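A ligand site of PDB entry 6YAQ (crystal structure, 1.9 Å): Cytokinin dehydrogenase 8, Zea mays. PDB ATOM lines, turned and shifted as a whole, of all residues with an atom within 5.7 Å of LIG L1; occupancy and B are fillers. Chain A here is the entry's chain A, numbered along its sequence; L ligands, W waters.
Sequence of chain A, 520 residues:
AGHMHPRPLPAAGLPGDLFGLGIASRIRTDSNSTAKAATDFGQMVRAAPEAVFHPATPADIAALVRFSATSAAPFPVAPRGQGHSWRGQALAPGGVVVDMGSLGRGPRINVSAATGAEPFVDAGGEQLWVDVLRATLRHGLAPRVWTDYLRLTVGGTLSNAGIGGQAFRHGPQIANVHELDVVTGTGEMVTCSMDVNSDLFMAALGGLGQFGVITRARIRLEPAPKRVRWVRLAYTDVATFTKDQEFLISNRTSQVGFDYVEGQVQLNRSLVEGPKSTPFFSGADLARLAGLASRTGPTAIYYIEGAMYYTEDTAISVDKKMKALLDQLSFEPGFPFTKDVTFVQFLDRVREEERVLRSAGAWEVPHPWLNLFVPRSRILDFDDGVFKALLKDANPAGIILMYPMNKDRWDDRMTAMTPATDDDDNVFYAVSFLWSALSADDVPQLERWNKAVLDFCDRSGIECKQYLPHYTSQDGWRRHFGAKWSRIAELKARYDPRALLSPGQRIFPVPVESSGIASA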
ATOM      1  N   PHE A  41      -8.354  27.316  -4.927  1.00  0.00           N
ATOM      2  CA  PHE A  41      -9.217  26.239  -4.422  1.00  0.00           C
ATOM      3  C   PHE A  41      -8.478  24.861  -4.300  1.00  0.00           C
ATOM      4  O   PHE A  41      -8.828  24.074  -3.422  1.00  0.00           O
ATOM      5  CB  PHE A  41     -10.503  26.154  -5.271  1.00  0.00           C
ATOM      6  CG  PHE A  41     -11.448  25.028  -4.932  1.00  0.00           C
ATOM      7  CD1 PHE A  41     -12.356  25.146  -3.878  1.00  0.00           C
ATOM      8  CD2 PHE A  41     -11.449  23.855  -5.679  1.00  0.00           C
ATOM      9  CE1 PHE A  41     -13.270  24.125  -3.601  1.00  0.00           C
ATOM     10  CE2 PHE A  41     -12.363  22.834  -5.402  1.00  0.00           C
ATOM     11  CZ  PHE A  41     -13.261  22.979  -4.363  1.00  0.00           C
ATOM     12  N   TRP A  86      -7.393  24.866  -9.573  1.00  0.00           N
ATOM     13  CA  TRP A  86      -6.631  24.060  -8.644  1.00  0.00           C
ATOM     14  C   TRP A  86      -5.197  23.775  -9.069  1.00  0.00           C
ATOM     15  O   TRP A  86      -4.507  23.022  -8.370  1.00  0.00           O
ATOM     16  CB  TRP A  86      -7.396  22.749  -8.306  1.00  0.00           C
ATOM     17  CG  TRP A  86      -8.066  22.079  -9.465  1.00  0.00           C
ATOM     18  CD1 TRP A  86      -7.558  21.086 -10.250  1.00  0.00           C
ATOM     19  CD2 TRP A  86      -9.385  22.344  -9.975  1.00  0.00           C
ATOM     20  NE1 TRP A  86      -8.466  20.735 -11.232  1.00  0.00           N
ATOM     21  CE2 TRP A  86      -9.588  21.493 -11.080  1.00  0.00           C
ATOM     22  CE3 TRP A  86     -10.418  23.226  -9.586  1.00  0.00           C
ATOM     23  CZ2 TRP A  86     -10.786  21.496 -11.813  1.00  0.00           C
ATOM     24  CZ3 TRP A  86     -11.602  23.220 -10.304  1.00  0.00           C
ATOM     25  CH2 TRP A  86     -11.787  22.354 -11.382  1.00  0.00           C
ATOM     26  N   ASP A 148     -22.322  23.542 -12.517  1.00  0.00           N
ATOM     27  CA  ASP A 148     -22.922  22.934 -11.331  1.00  0.00           C
ATOM     28  C   ASP A 148     -22.821  23.865 -10.112  1.00  0.00           C
ATOM     29  O   ASP A 148     -23.656  23.767  -9.239  1.00  0.00           O
ATOM     30  CB  ASP A 148     -22.243  21.602 -10.984  1.00  0.00           C
ATOM     31  CG  ASP A 148     -22.339  20.510 -12.022  1.00  0.00           C
ATOM     32  OD1 ASP A 148     -23.280  20.554 -12.861  1.00  0.00           O
ATOM     33  OD2 ASP A 148     -21.504  19.592 -11.988  1.00  0.00           O
ATOM     34  N   TYR A 149     -21.772  24.709 -10.042  1.00  0.00           N
ATOM     35  CA  TYR A 149     -21.512  25.651  -8.939  1.00  0.00           C
ATOM     36  C   TYR A 149     -21.687  27.083  -9.473  1.00  0.00           C
ATOM     37  O   TYR A 149     -20.998  27.463 -10.413  1.00  0.00           O
ATOM     38  CB  TYR A 149     -20.070  25.411  -8.422  1.00  0.00           C
ATOM     39  CG  TYR A 149     -19.689  26.173  -7.175  1.00  0.00           C
ATOM     40  CD1 TYR A 149     -20.244  25.848  -5.944  1.00  0.00           C
ATOM     41  CD2 TYR A 149     -18.687  27.146  -7.207  1.00  0.00           C
ATOM     42  CE1 TYR A 149     -19.873  26.534  -4.786  1.00  0.00           C
ATOM     43  CE2 TYR A 149     -18.312  27.838  -6.056  1.00  0.00           C
ATOM     44  CZ  TYR A 149     -18.912  27.518  -4.846  1.00  0.00           C
ATOM     45  OH  TYR A 149     -18.540  28.153  -3.704  1.00  0.00           O
ATOM     46  N   ILE A 163     -19.272  23.911 -18.579  1.00  0.00           N
ATOM     47  CA  ILE A 163     -20.066  22.703 -18.827  1.00  0.00           C
ATOM     48  C   ILE A 163     -21.033  22.449 -17.672  1.00  0.00           C
ATOM     49  O   ILE A 163     -20.814  22.898 -16.537  1.00  0.00           O
ATOM     50  CB  ILE A 163     -19.203  21.440 -19.189  1.00  0.00           C
ATOM     51  CG1 ILE A 163     -18.375  20.921 -17.978  1.00  0.00           C
ATOM     52  CG2 ILE A 163     -18.312  21.706 -20.436  1.00  0.00           C
ATOM     53  CD1 ILE A 163     -17.771  19.525 -18.113  1.00  0.00           C
ATOM     54  N   GLY A 164     -22.106  21.722 -17.989  1.00  0.00           N
ATOM     55  CA  GLY A 164     -23.151  21.367 -17.045  1.00  0.00           C
ATOM     56  C   GLY A 164     -24.222  20.545 -17.711  1.00  0.00           C
ATOM     57  O   GLY A 164     -24.096  20.227 -18.906  1.00  0.00           O
ATOM     58  N   ARG A 232     -32.838  11.212  -9.260  1.00  0.00           N
ATOM     59  CA  ARG A 232     -31.626  10.384  -9.290  1.00  0.00           C
ATOM     60  C   ARG A 232     -32.134   8.951  -9.468  1.00  0.00           C
ATOM     61  O   ARG A 232     -33.039   8.503  -8.745  1.00  0.00           O
ATOM     62  CB  ARG A 232     -30.745  10.555  -8.044  1.00  0.00           C
ATOM     63  CG  ARG A 232     -29.959  11.852  -8.103  1.00  0.00           C
ATOM     64  CD  ARG A 232     -28.893  11.968  -7.047  1.00  0.00           C
ATOM     65  NE  ARG A 232     -28.321  13.309  -7.046  1.00  0.00           N
ATOM     66  CZ  ARG A 232     -27.460  13.775  -6.149  1.00  0.00           C
ATOM     67  NH1 ARG A 232     -27.005  15.020  -6.230  1.00  0.00           N
ATOM     68  NH2 ARG A 232     -27.050  12.997  -5.153  1.00  0.00           N
ATOM     69  N   GLU A 262     -27.224  14.624 -16.068  1.00  0.00           N
ATOM     70  CA  GLU A 262     -25.887  14.336 -15.554  1.00  0.00           C
ATOM     71  C   GLU A 262     -25.878  12.893 -15.025  1.00  0.00           C
ATOM     72  O   GLU A 262     -26.861  12.142 -15.163  1.00  0.00           O
ATOM     73  CB  GLU A 262     -25.424  15.353 -14.483  1.00  0.00           C
ATOM     74  CG  GLU A 262     -25.041  16.704 -15.084  1.00  0.00           C
ATOM     75  CD  GLU A 262     -24.184  17.653 -14.268  1.00  0.00           C
ATOM     76  OE1 GLU A 262     -24.031  18.797 -14.721  1.00  0.00           O
ATOM     77  OE2 GLU A 262     -23.669  17.259 -13.188  1.00  0.00           O
ATOM     78  N   ARG A 349     -28.112  24.296  -5.943  1.00  0.00           N
ATOM     79  CA  ARG A 349     -28.031  23.061  -5.141  1.00  0.00           C
ATOM     80  C   ARG A 349     -26.659  22.812  -4.483  1.00  0.00           C
ATOM     81  O   ARG A 349     -26.633  22.307  -3.365  1.00  0.00           O
ATOM     82  CB  ARG A 349     -28.477  21.806  -5.959  1.00  0.00           C
ATOM     83  CG  ARG A 349     -27.490  21.317  -7.036  1.00  0.00           C
ATOM     84  CD  ARG A 349     -28.134  20.494  -8.170  1.00  0.00           C
ATOM     85  NE  ARG A 349     -27.166  20.202  -9.227  1.00  0.00           N
ATOM     86  CZ  ARG A 349     -26.850  21.044 -10.207  1.00  0.00           C
ATOM     87  NH1 ARG A 349     -27.447  22.231 -10.300  1.00  0.00           N
ATOM     88  NH2 ARG A 349     -25.922  20.719 -11.098  1.00  0.00           N
ATOM     89  N   VAL A 350     -25.540  23.145  -5.168  1.00  0.00           N
ATOM     90  CA  VAL A 350     -24.186  22.867  -4.664  1.00  0.00           C
ATOM     91  C   VAL A 350     -23.845  23.803  -3.475  1.00  0.00           C
ATOM     92  O   VAL A 350     -23.070  23.384  -2.616  1.00  0.00           O
ATOM     93  CB  VAL A 350     -23.104  22.827  -5.780  1.00  0.00           C
ATOM     94  CG1 VAL A 350     -21.699  22.567  -5.215  1.00  0.00           C
ATOM     95  CG2 VAL A 350     -23.449  21.744  -6.810  1.00  0.00           C
ATOM     96  N   GLU A 353     -24.399  21.824  -0.456  1.00  0.00           N
ATOM     97  CA  GLU A 353     -23.338  20.832  -0.282  1.00  0.00           C
ATOM     98  C   GLU A 353     -22.111  21.526   0.331  1.00  0.00           C
ATOM     99  O   GLU A 353     -21.475  20.974   1.237  1.00  0.00           O
ATOM    100  CB  GLU A 353     -22.944  20.170  -1.629  1.00  0.00           C
ATOM    101  CG  GLU A 353     -24.111  19.743  -2.510  1.00  0.00           C
ATOM    102  CD  GLU A 353     -24.374  18.257  -2.606  1.00  0.00           C
ATOM    103  OE1 GLU A 353     -25.478  17.825  -2.206  1.00  0.00           O
ATOM    104  OE2 GLU A 353     -23.487  17.519  -3.098  1.00  0.00           O
ATOM    105  N   GLU A 354     -21.777  22.741  -0.156  1.00  0.00           N
ATOM    106  CA  GLU A 354     -20.656  23.538   0.355  1.00  0.00           C
ATOM    107  C   GLU A 354     -20.829  23.869   1.857  1.00  0.00           C
ATOM    108  O   GLU A 354     -19.881  23.747   2.615  1.00  0.00           O
ATOM    109  CB  GLU A 354     -20.491  24.829  -0.457  1.00  0.00           C
ATOM    110  CG  GLU A 354     -19.426  25.765   0.087  1.00  0.00           C
ATOM    111  CD  GLU A 354     -19.256  27.090  -0.633  1.00  0.00           C
ATOM    112  OE1 GLU A 354     -20.028  27.381  -1.575  1.00  0.00           O
ATOM    113  OE2 GLU A 354     -18.352  27.855  -0.235  1.00  0.00           O
ATOM    114  N   LEU A 357     -20.113  20.741   3.886  1.00  0.00           N
ATOM    115  CA  LEU A 357     -18.677  20.494   3.835  1.00  0.00           C
ATOM    116  C   LEU A 357     -17.883  21.469   4.696  1.00  0.00           C
ATOM    117  O   LEU A 357     -16.973  21.050   5.414  1.00  0.00           O
ATOM    118  CB  LEU A 357     -18.167  20.466   2.379  1.00  0.00           C
ATOM    119  CG  LEU A 357     -18.575  19.219   1.531  1.00  0.00           C
ATOM    120  CD1 LEU A 357     -18.413  19.492   0.037  1.00  0.00           C
ATOM    121  CD2 LEU A 357     -17.788  17.974   1.932  1.00  0.00           C
ATOM    122  N   TRP A 363     -14.168  21.406   3.232  1.00  0.00           N
ATOM    123  CA  TRP A 363     -14.238  22.242   2.034  1.00  0.00           C
ATOM    124  C   TRP A 363     -12.872  22.864   1.739  1.00  0.00           C
ATOM    125  O   TRP A 363     -12.393  22.727   0.621  1.00  0.00           O
ATOM    126  CB  TRP A 363     -15.318  23.328   2.154  1.00  0.00           C
ATOM    127  CG  TRP A 363     -15.471  24.181   0.922  1.00  0.00           C
ATOM    128  CD1 TRP A 363     -14.835  25.366   0.658  1.00  0.00           C
ATOM    129  CD2 TRP A 363     -16.258  23.887  -0.248  1.00  0.00           C
ATOM    130  NE1 TRP A 363     -15.211  25.844  -0.573  1.00  0.00           N
ATOM    131  CE2 TRP A 363     -16.088  24.964  -1.147  1.00  0.00           C
ATOM    132  CE3 TRP A 363     -17.106  22.823  -0.603  1.00  0.00           C
ATOM    133  CZ2 TRP A 363     -16.745  25.010  -2.388  1.00  0.00           C
ATOM    134  CZ3 TRP A 363     -17.756  22.876  -1.834  1.00  0.00           C
ATOM    135  CH2 TRP A 363     -17.571  23.967  -2.712  1.00  0.00           C
ATOM    136  N   HIS A 367      -7.688  19.965  -3.390  1.00  0.00           N
ATOM    137  CA  HIS A 367      -8.567  19.413  -4.434  1.00  0.00           C
ATOM    138  C   HIS A 367      -7.746  19.044  -5.691  1.00  0.00           C
ATOM    139  O   HIS A 367      -7.715  19.816  -6.653  1.00  0.00           O
ATOM    140  CB  HIS A 367      -9.722  20.358  -4.794  1.00  0.00           C
ATOM    141  CG  HIS A 367     -10.587  20.691  -3.639  1.00  0.00           C
ATOM    142  ND1 HIS A 367     -10.409  21.858  -2.911  1.00  0.00           N
ATOM    143  CD2 HIS A 367     -11.613  19.991  -3.096  1.00  0.00           C
ATOM    144  CE1 HIS A 367     -11.318  21.826  -1.963  1.00  0.00           C
ATOM    145  NE2 HIS A 367     -12.064  20.722  -2.030  1.00  0.00           N
ATOM    146  N   TRP A 369      -8.133  17.694  -8.411  1.00  0.00           N
ATOM    147  CA  TRP A 369      -9.198  17.334  -9.347  1.00  0.00           C
ATOM    148  C   TRP A 369      -8.664  17.034 -10.756  1.00  0.00           C
ATOM    149  O   TRP A 369      -7.590  17.516 -11.129  1.00  0.00           O
ATOM    150  CB  TRP A 369     -10.280  18.419  -9.362  1.00  0.00           C
ATOM    151  CG  TRP A 369     -11.153  18.493  -8.137  1.00  0.00           C
ATOM    152  CD1 TRP A 369     -11.038  17.755  -6.985  1.00  0.00           C
ATOM    153  CD2 TRP A 369     -12.285  19.356  -7.940  1.00  0.00           C
ATOM    154  NE1 TRP A 369     -12.063  18.057  -6.129  1.00  0.00           N
ATOM    155  CE2 TRP A 369     -12.834  19.054  -6.670  1.00  0.00           C
ATOM    156  CE3 TRP A 369     -12.911  20.329  -8.741  1.00  0.00           C
ATOM    157  CZ2 TRP A 369     -13.970  19.701  -6.171  1.00  0.00           C
ATOM    158  CZ3 TRP A 369     -14.038  20.974  -8.238  1.00  0.00           C
ATOM    159  CH2 TRP A 369     -14.572  20.648  -6.981  1.00  0.00           C
ATOM    160  N   ASN A 371     -10.397  16.444 -14.804  1.00  0.00           N
ATOM    161  CA  ASN A 371     -11.588  16.466 -15.662  1.00  0.00           C
ATOM    162  C   ASN A 371     -11.207  16.003 -17.073  1.00  0.00           C
ATOM    163  O   ASN A 371     -10.315  16.575 -17.693  1.00  0.00           O
ATOM    164  CB  ASN A 371     -12.225  17.858 -15.668  1.00  0.00           C
ATOM    165  CG  ASN A 371     -12.680  18.294 -14.296  1.00  0.00           C
ATOM    166  OD1 ASN A 371     -13.815  18.047 -13.880  1.00  0.00           O
ATOM    167  ND2 ASN A 371     -11.796  18.927 -13.543  1.00  0.00           N
ATOM    168  N   ILE A 399     -16.611  13.397  -5.071  1.00  0.00           N
ATOM    169  CA  ILE A 399     -17.490  12.666  -5.996  1.00  0.00           C
ATOM    170  C   ILE A 399     -16.844  12.425  -7.345  1.00  0.00           C
ATOM    171  O   ILE A 399     -15.841  13.062  -7.693  1.00  0.00           O
ATOM    172  CB  ILE A 399     -18.862  13.390  -6.169  1.00  0.00           C
ATOM    173  CG1 ILE A 399     -18.676  14.855  -6.680  1.00  0.00           C
ATOM    174  CG2 ILE A 399     -19.749  13.296  -4.911  1.00  0.00           C
ATOM    175  CD1 ILE A 399     -19.973  15.521  -7.139  1.00  0.00           C
ATOM    176  N   LEU A 401     -18.204  12.400 -11.310  1.00  0.00           N
ATOM    177  CA  LEU A 401     -19.295  12.661 -12.248  1.00  0.00           C
ATOM    178  C   LEU A 401     -19.009  12.050 -13.613  1.00  0.00           C
ATOM    179  O   LEU A 401     -17.854  11.929 -14.024  1.00  0.00           O
ATOM    180  CB  LEU A 401     -19.673  14.167 -12.321  1.00  0.00           C
ATOM    181  CG  LEU A 401     -20.069  14.837 -10.968  1.00  0.00           C
ATOM    182  CD1 LEU A 401     -20.310  16.315 -11.147  1.00  0.00           C
ATOM    183  CD2 LEU A 401     -21.296  14.166 -10.327  1.00  0.00           C
ATOM    184  N   TYR A 403     -21.201  11.822 -17.547  1.00  0.00           N
ATOM    185  CA  TYR A 403     -22.362  12.026 -18.400  1.00  0.00           C
ATOM    186  C   TYR A 403     -21.944  12.401 -19.843  1.00  0.00           C
ATOM    187  O   TYR A 403     -20.868  12.965 -20.037  1.00  0.00           O
ATOM    188  CB  TYR A 403     -23.355  13.066 -17.801  1.00  0.00           C
ATOM    189  CG  TYR A 403     -22.776  14.447 -17.598  1.00  0.00           C
ATOM    190  CD1 TYR A 403     -22.099  14.773 -16.422  1.00  0.00           C
ATOM    191  CD2 TYR A 403     -22.876  15.423 -18.586  1.00  0.00           C
ATOM    192  CE1 TYR A 403     -21.573  16.047 -16.229  1.00  0.00           C
ATOM    193  CE2 TYR A 403     -22.339  16.701 -18.413  1.00  0.00           C
ATOM    194  CZ  TYR A 403     -21.698  17.012 -17.212  1.00  0.00           C
ATOM    195  OH  TYR A 403     -21.137  18.251 -17.030  1.00  0.00           O
ATOM    196  N   SER A 432     -15.529  13.453 -14.440  1.00  0.00           N
ATOM    197  CA  SER A 432     -14.914  14.396 -13.494  1.00  0.00           C
ATOM    198  C   SER A 432     -14.534  13.721 -12.203  1.00  0.00           C
ATOM    199  O   SER A 432     -15.406  13.224 -11.490  1.00  0.00           O
ATOM    200  CB  SER A 432     -15.848  15.583 -13.256  1.00  0.00           C
ATOM    201  OG  SER A 432     -16.179  16.227 -14.472  1.00  0.00           O
ATOM    202  N   LEU A 434     -13.655  14.534  -8.898  1.00  0.00           N
ATOM    203  CA  LEU A 434     -13.709  15.636  -7.940  1.00  0.00           C
ATOM    204  C   LEU A 434     -13.424  15.104  -6.532  1.00  0.00           C
ATOM    205  O   LEU A 434     -14.241  15.235  -5.618  1.00  0.00           O
ATOM    206  CB  LEU A 434     -15.059  16.370  -8.017  1.00  0.00           C
ATOM    207  CG  LEU A 434     -15.583  16.665  -9.426  1.00  0.00           C
ATOM    208  CD1 LEU A 434     -16.982  17.180  -9.362  1.00  0.00           C
ATOM    209  CD2 LEU A 434     -14.626  17.604 -10.206  1.00  0.00           C
ATOM    210  N   SER A 436     -11.321  14.916  -3.024  1.00  0.00           N
ATOM    211  CA  SER A 436     -10.668  15.831  -2.095  1.00  0.00           C
ATOM    212  C   SER A 436      -9.816  15.096  -1.079  1.00  0.00           C
ATOM    213  O   SER A 436     -10.135  13.956  -0.721  1.00  0.00           O
ATOM    214  CB  SER A 436     -11.723  16.686  -1.390  1.00  0.00           C
ATOM    215  OG  SER A 436     -12.681  17.164  -2.318  1.00  0.00           O
ATOM    216  N   TYR A 467     -10.384  18.694 -19.645  1.00  0.00           N
ATOM    217  CA  TYR A 467     -11.168  19.924 -19.501  1.00  0.00           C
ATOM    218  C   TYR A 467     -10.444  20.606 -18.358  1.00  0.00           C
ATOM    219  O   TYR A 467      -9.954  19.888 -17.467  1.00  0.00           O
ATOM    220  CB  TYR A 467     -12.645  19.665 -19.165  1.00  0.00           C
ATOM    221  CG  TYR A 467     -13.439  20.932 -18.921  1.00  0.00           C
ATOM    222  CD1 TYR A 467     -13.407  21.999 -19.836  1.00  0.00           C
ATOM    223  CD2 TYR A 467     -14.219  21.079 -17.780  1.00  0.00           C
ATOM    224  CE1 TYR A 467     -14.083  23.185 -19.580  1.00  0.00           C
ATOM    225  CE2 TYR A 467     -14.926  22.261 -17.530  1.00  0.00           C
ATOM    226  CZ  TYR A 467     -14.870  23.304 -18.454  1.00  0.00           C
ATOM    227  OH  TYR A 467     -15.542  24.473 -18.210  1.00  0.00           O
ATOM    228  N   LEU A 468     -10.267  21.953 -18.394  1.00  0.00           N
ATOM    229  CA  LEU A 468      -9.429  22.720 -17.445  1.00  0.00           C
ATOM    230  C   LEU A 468      -7.999  22.102 -17.480  1.00  0.00           C
ATOM    231  O   LEU A 468      -7.491  21.598 -16.459  1.00  0.00           O
ATOM    232  CB  LEU A 468     -10.047  22.754 -16.017  1.00  0.00           C
ATOM    233  CG  LEU A 468     -11.562  22.981 -16.016  1.00  0.00           C
ATOM    234  CD1 LEU A 468     -12.222  22.256 -14.898  1.00  0.00           C
ATOM    235  CD2 LEU A 468     -11.910  24.428 -16.051  1.00  0.00           C
HETATM  236  C1  LIG L   1     -20.213  19.331  -8.275  1.00  0.00           C
HETATM  237  C2  LIG L   1     -21.488  18.867  -7.991  1.00  0.00           C
HETATM  238  C3  LIG L   1     -21.810  18.512  -6.694  1.00  0.00           C
HETATM  239  C4  LIG L   1     -20.889  18.612  -5.664  1.00  0.00           C
HETATM  240  C5  LIG L   1     -19.606  19.045  -5.972  1.00  0.00           C
HETATM  241  C6  LIG L   1     -18.318  19.907  -4.173  1.00  0.00           C
HETATM  242  C7  LIG L   1     -19.263  19.434  -7.256  1.00  0.00           C
HETATM  243  C8  LIG L   1     -16.147  20.619 -11.636  1.00  0.00           C
HETATM  244  C9  LIG L   1     -15.071  20.986 -12.433  1.00  0.00           C
HETATM  245  C10 LIG L   1     -15.194  20.966 -13.801  1.00  0.00           C
HETATM  246  C11 LIG L   1     -16.384  20.561 -14.397  1.00  0.00           C
HETATM  247  C12 LIG L   1     -18.764  19.770 -14.310  1.00  0.00           C
HETATM  248  F1  LIG L   1     -19.328  20.084  -3.333  1.00  0.00           F
HETATM  249  F2  LIG L   1     -17.250  19.623  -3.447  1.00  0.00           F
HETATM  250  F3  LIG L   1     -18.107  21.061  -4.788  1.00  0.00           F
HETATM  251  O1  LIG L   1     -18.565  18.901  -5.018  1.00  0.00           O
HETATM  252 CL1  LIG L   1     -23.382  17.866  -6.351  1.00  0.00          CL
HETATM  253  N1  LIG L   1     -19.853  19.627  -9.618  1.00  0.00           N
HETATM  254  C13 LIG L   1     -18.658  20.136 -10.071  1.00  0.00           C
HETATM  255  O2  LIG L   1     -17.783  20.604  -9.340  1.00  0.00           O
HETATM  256  N2  LIG L   1     -18.522  19.992 -11.427  1.00  0.00           N
HETATM  257  C14 LIG L   1     -17.360  20.239 -12.223  1.00  0.00           C
HETATM  258  C15 LIG L   1     -17.474  20.180 -13.620  1.00  0.00           C
HETATM  259  C16 LIG L   1     -19.040  18.278 -14.198  1.00  0.00           C
HETATM  260  O3  LIG L   1     -20.441  18.067 -14.054  1.00  0.00           O
HETATM  261  P1  LG2 L   2     -10.179  31.723 -11.467  1.00  0.00           P
HETATM  262  O1  LG2 L   2     -10.059  30.439 -10.759  1.00  0.00           O
HETATM  263  O2  LG2 L   2      -9.944  32.874 -10.514  1.00  0.00           O
HETATM  264  O3  LG2 L   2      -9.259  31.831 -12.766  1.00  0.00           O
HETATM  265  C1  LG2 L   2      -9.091  30.682 -13.626  1.00  0.00           C
HETATM  266  C2  LG2 L   2      -8.260  31.060 -14.837  1.00  0.00           C
HETATM  267  O4  LG2 L   2      -9.017  31.949 -15.688  1.00  0.00           O
HETATM  268  C3  LG2 L   2      -6.936  31.775 -14.559  1.00  0.00           C
HETATM  269  O5  LG2 L   2      -5.976  31.439 -15.543  1.00  0.00           O
HETATM  270  C4  LG2 L   2      -7.347  33.252 -14.619  1.00  0.00           C
HETATM  271  O6  LG2 L   2      -6.281  34.175 -14.819  1.00  0.00           O
HETATM  272  C5  LG2 L   2      -8.377  33.217 -15.756  1.00  0.00           C
HETATM  273  N1  LG2 L   2      -9.402  34.256 -15.691  1.00  0.00           N
HETATM  274  C6  LG2 L   2     -10.210  34.575 -14.633  1.00  0.00           C
HETATM  275  N2  LG2 L   2     -11.079  35.526 -14.892  1.00  0.00           N
HETATM  276  C7  LG2 L   2     -10.803  35.872 -16.209  1.00  0.00           C
HETATM  277  C8  LG2 L   2     -11.343  36.850 -17.072  1.00  0.00           C
HETATM  278  N3  LG2 L   2     -12.294  37.725 -16.715  1.00  0.00           N
HETATM  279  N4  LG2 L   2     -10.836  36.929 -18.333  1.00  0.00           N
HETATM  280  C9  LG2 L   2      -9.849  36.107 -18.681  1.00  0.00           C
HETATM  281  N5  LG2 L   2      -9.244  35.154 -17.947  1.00  0.00           N
HETATM  282  C10 LG2 L   2      -9.778  35.092 -16.718  1.00  0.00           C
HETATM  283  N6  LG2 L   2     -16.462  24.307 -14.379  1.00  0.00           N
HETATM  284  C11 LG2 L   2     -17.466  23.929 -15.238  1.00  0.00           C
HETATM  285  O7  LG2 L   2     -17.425  24.160 -16.445  1.00  0.00           O
HETATM  286  N7  LG2 L   2     -18.619  23.339 -14.730  1.00  0.00           N
HETATM  287  C12 LG2 L   2     -18.874  23.091 -13.385  1.00  0.00           C
HETATM  288  O8  LG2 L   2     -19.913  22.516 -13.062  1.00  0.00           O
HETATM  289  C13 LG2 L   2     -17.818  23.515 -12.484  1.00  0.00           C
HETATM  290  N8  LG2 L   2     -18.000  23.345 -11.202  1.00  0.00           N
HETATM  291  C14 LG2 L   2     -17.000  23.796 -10.340  1.00  0.00           C
HETATM  292  C15 LG2 L   2     -17.212  23.652  -8.965  1.00  0.00           C
HETATM  293  C16 LG2 L   2     -16.295  24.148  -8.037  1.00  0.00           C
HETATM  294  C17 LG2 L   2     -16.551  23.923  -6.569  1.00  0.00           C
HETATM  295  C18 LG2 L   2     -15.125  24.796  -8.497  1.00  0.00           C
HETATM  296  C19 LG2 L   2     -14.099  25.328  -7.532  1.00  0.00           C
HETATM  297  C20 LG2 L   2     -14.913  24.918  -9.877  1.00  0.00           C
HETATM  298  C21 LG2 L   2     -15.830  24.422 -10.805  1.00  0.00           C
HETATM  299  N9  LG2 L   2     -15.650  24.555 -12.209  1.00  0.00           N
HETATM  300  C22 LG2 L   2     -16.634  24.123 -13.075  1.00  0.00           C
HETATM  301  C23 LG2 L   2     -14.412  25.144 -12.756  1.00  0.00           C
HETATM  302  C24 LG2 L   2     -14.466  26.618 -13.137  1.00  0.00           C
HETATM  303  O9  LG2 L   2     -15.409  26.820 -14.186  1.00  0.00           O
HETATM  304  C25 LG2 L   2     -13.129  27.135 -13.674  1.00  0.00           C
HETATM  305  O10 LG2 L   2     -12.078  26.704 -12.811  1.00  0.00           O
HETATM  306  C26 LG2 L   2     -13.076  28.615 -14.046  1.00  0.00           C
HETATM  307  O11 LG2 L   2     -11.733  29.068 -14.124  1.00  0.00           O
HETATM  308  C27 LG2 L   2     -13.941  29.544 -13.207  1.00  0.00           C
HETATM  309  O12 LG2 L   2     -13.319  29.939 -11.971  1.00  0.00           O
HETATM  310  P2  LG2 L   2     -13.092  31.526 -11.496  1.00  0.00           P
HETATM  311  O13 LG2 L   2     -14.015  32.661 -11.711  1.00  0.00           O
HETATM  312  O14 LG2 L   2     -12.927  31.340 -10.010  1.00  0.00           O
HETATM  313  O15 LG2 L   2     -11.651  31.896 -12.076  1.00  0.00           O
HETATM  314  O   HOH W   1     -23.859  18.217 -10.340  1.00  0.00           O
HETATM  315  O   HOH W   2     -26.126  17.550  -8.400  1.00  0.00           O
HETATM  316  O   HOH W   3     -26.542  17.971  -5.726  1.00  0.00           O
HETATM  317  O   HOH W   4     -15.484  17.452  -1.347  1.00  0.00           O
HETATM  318  O   HOH W   5     -18.476  15.178 -15.522  1.00  0.00           O
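The side-chain carboxylate (OD2) of Asp 148 lies within hydrogen-bond range of an oxygen (O3) of LIG L1, 2.8 Å away.
OH of Tyr 403 sits at hydrogen-bond distance from O3 of LIG L1, at 3.1 Å.
OE2 of Glu 262 sits at hydrogen-bond distance from O3 of LIG L1 (3.4 Å).
An oxygen (O8) of LG2 L2 sits at hydrogen-bond distance from the backbone NH of Asp 148 (2.7 Å).
An oxygen (O7) of LG2 L2 lies within hydrogen-bond range of the side-chain hydroxyl (OH) of Tyr 467 (2.6 Å).
The backbone NH (N) of Ile 163 lies within hydrogen-bond range of an oxygen (O7) of LG2 L2, 2.8 Å away.
The backbone carbonyl oxygen of Ile 163 sits at hydrogen-bond distance from a nitrogen (N7) of LG2 L2 (2.9 Å).
O8 of LG2 L2 lies close to N2 of LIG L1 (3.3 Å).
OE1 of Glu 262 lies close to OD1 of Asp 148 (2.7 Å).
OD1 of Asp 148 is in salt-bridge range of NH2 of Arg 349 (3.2 Å).
OD1 of Asn 371 is in hydrogen-bond range of OG of Ser 432 (3.0 Å).
N of Tyr 467 lies within hydrogen-bond range of O of Asn 371 (2.9 Å).
The backbone carbonyl oxygen of Leu 401 sits at hydrogen-bond distance from the backbone NH of Ser 432, 2.8 Å away.
N of Leu 434 sits at hydrogen-bond distance from O of Ile 399 (2.9 Å).
The backbone carbonyl oxygen (O) of Trp 363 lies close to a ring nitrogen (NE2) of His 367 (3.3 Å).
The backbone carbonyl oxygen (O) of Trp 369 lies within hydrogen-bond range of the indole nitrogen (NE1) of Trp 86 (3.3 Å).
Residues that only touch LIG L1: Trp 86 (3.7 Å), Ile 163 (3.9 Å), Val 350 (3.6 Å), Glu 353 (3.3 Å), Leu 357 (3.5 Å), Trp 363 (3.5 Å), Trp 369 (3.9 Å), Asn 371 (3.2 Å), Ile 399 (3.5 Å), Leu 401 (3.4 Å), Ser 432 (3.5 Å), Leu 434 (3.5 Å), Tyr 467 (3.9 Å) and Leu 468 (3.4 Å).
17 residues have an atom within 4 Å of LIG L1: Trp 86, Asp 148, Ile 163, Glu 262, Val 350, Glu 353, Leu 357, Trp 363, Trp 369, Asn 371, Ile 399, Leu 401, Tyr 403, Ser 432, Leu 434, Tyr 467 and Leu 468.
Water W1 lies within hydrogen-bond range of OE2 of Glu 262 (3.0 Å), OD2 of Asp 148 (3.2 Å) and NH2 of Arg 349 (3.3 Å).
Water W2 lies within hydrogen-bond range of the guanidinium group of Arg 349 and the guanidinium group of Arg 232.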
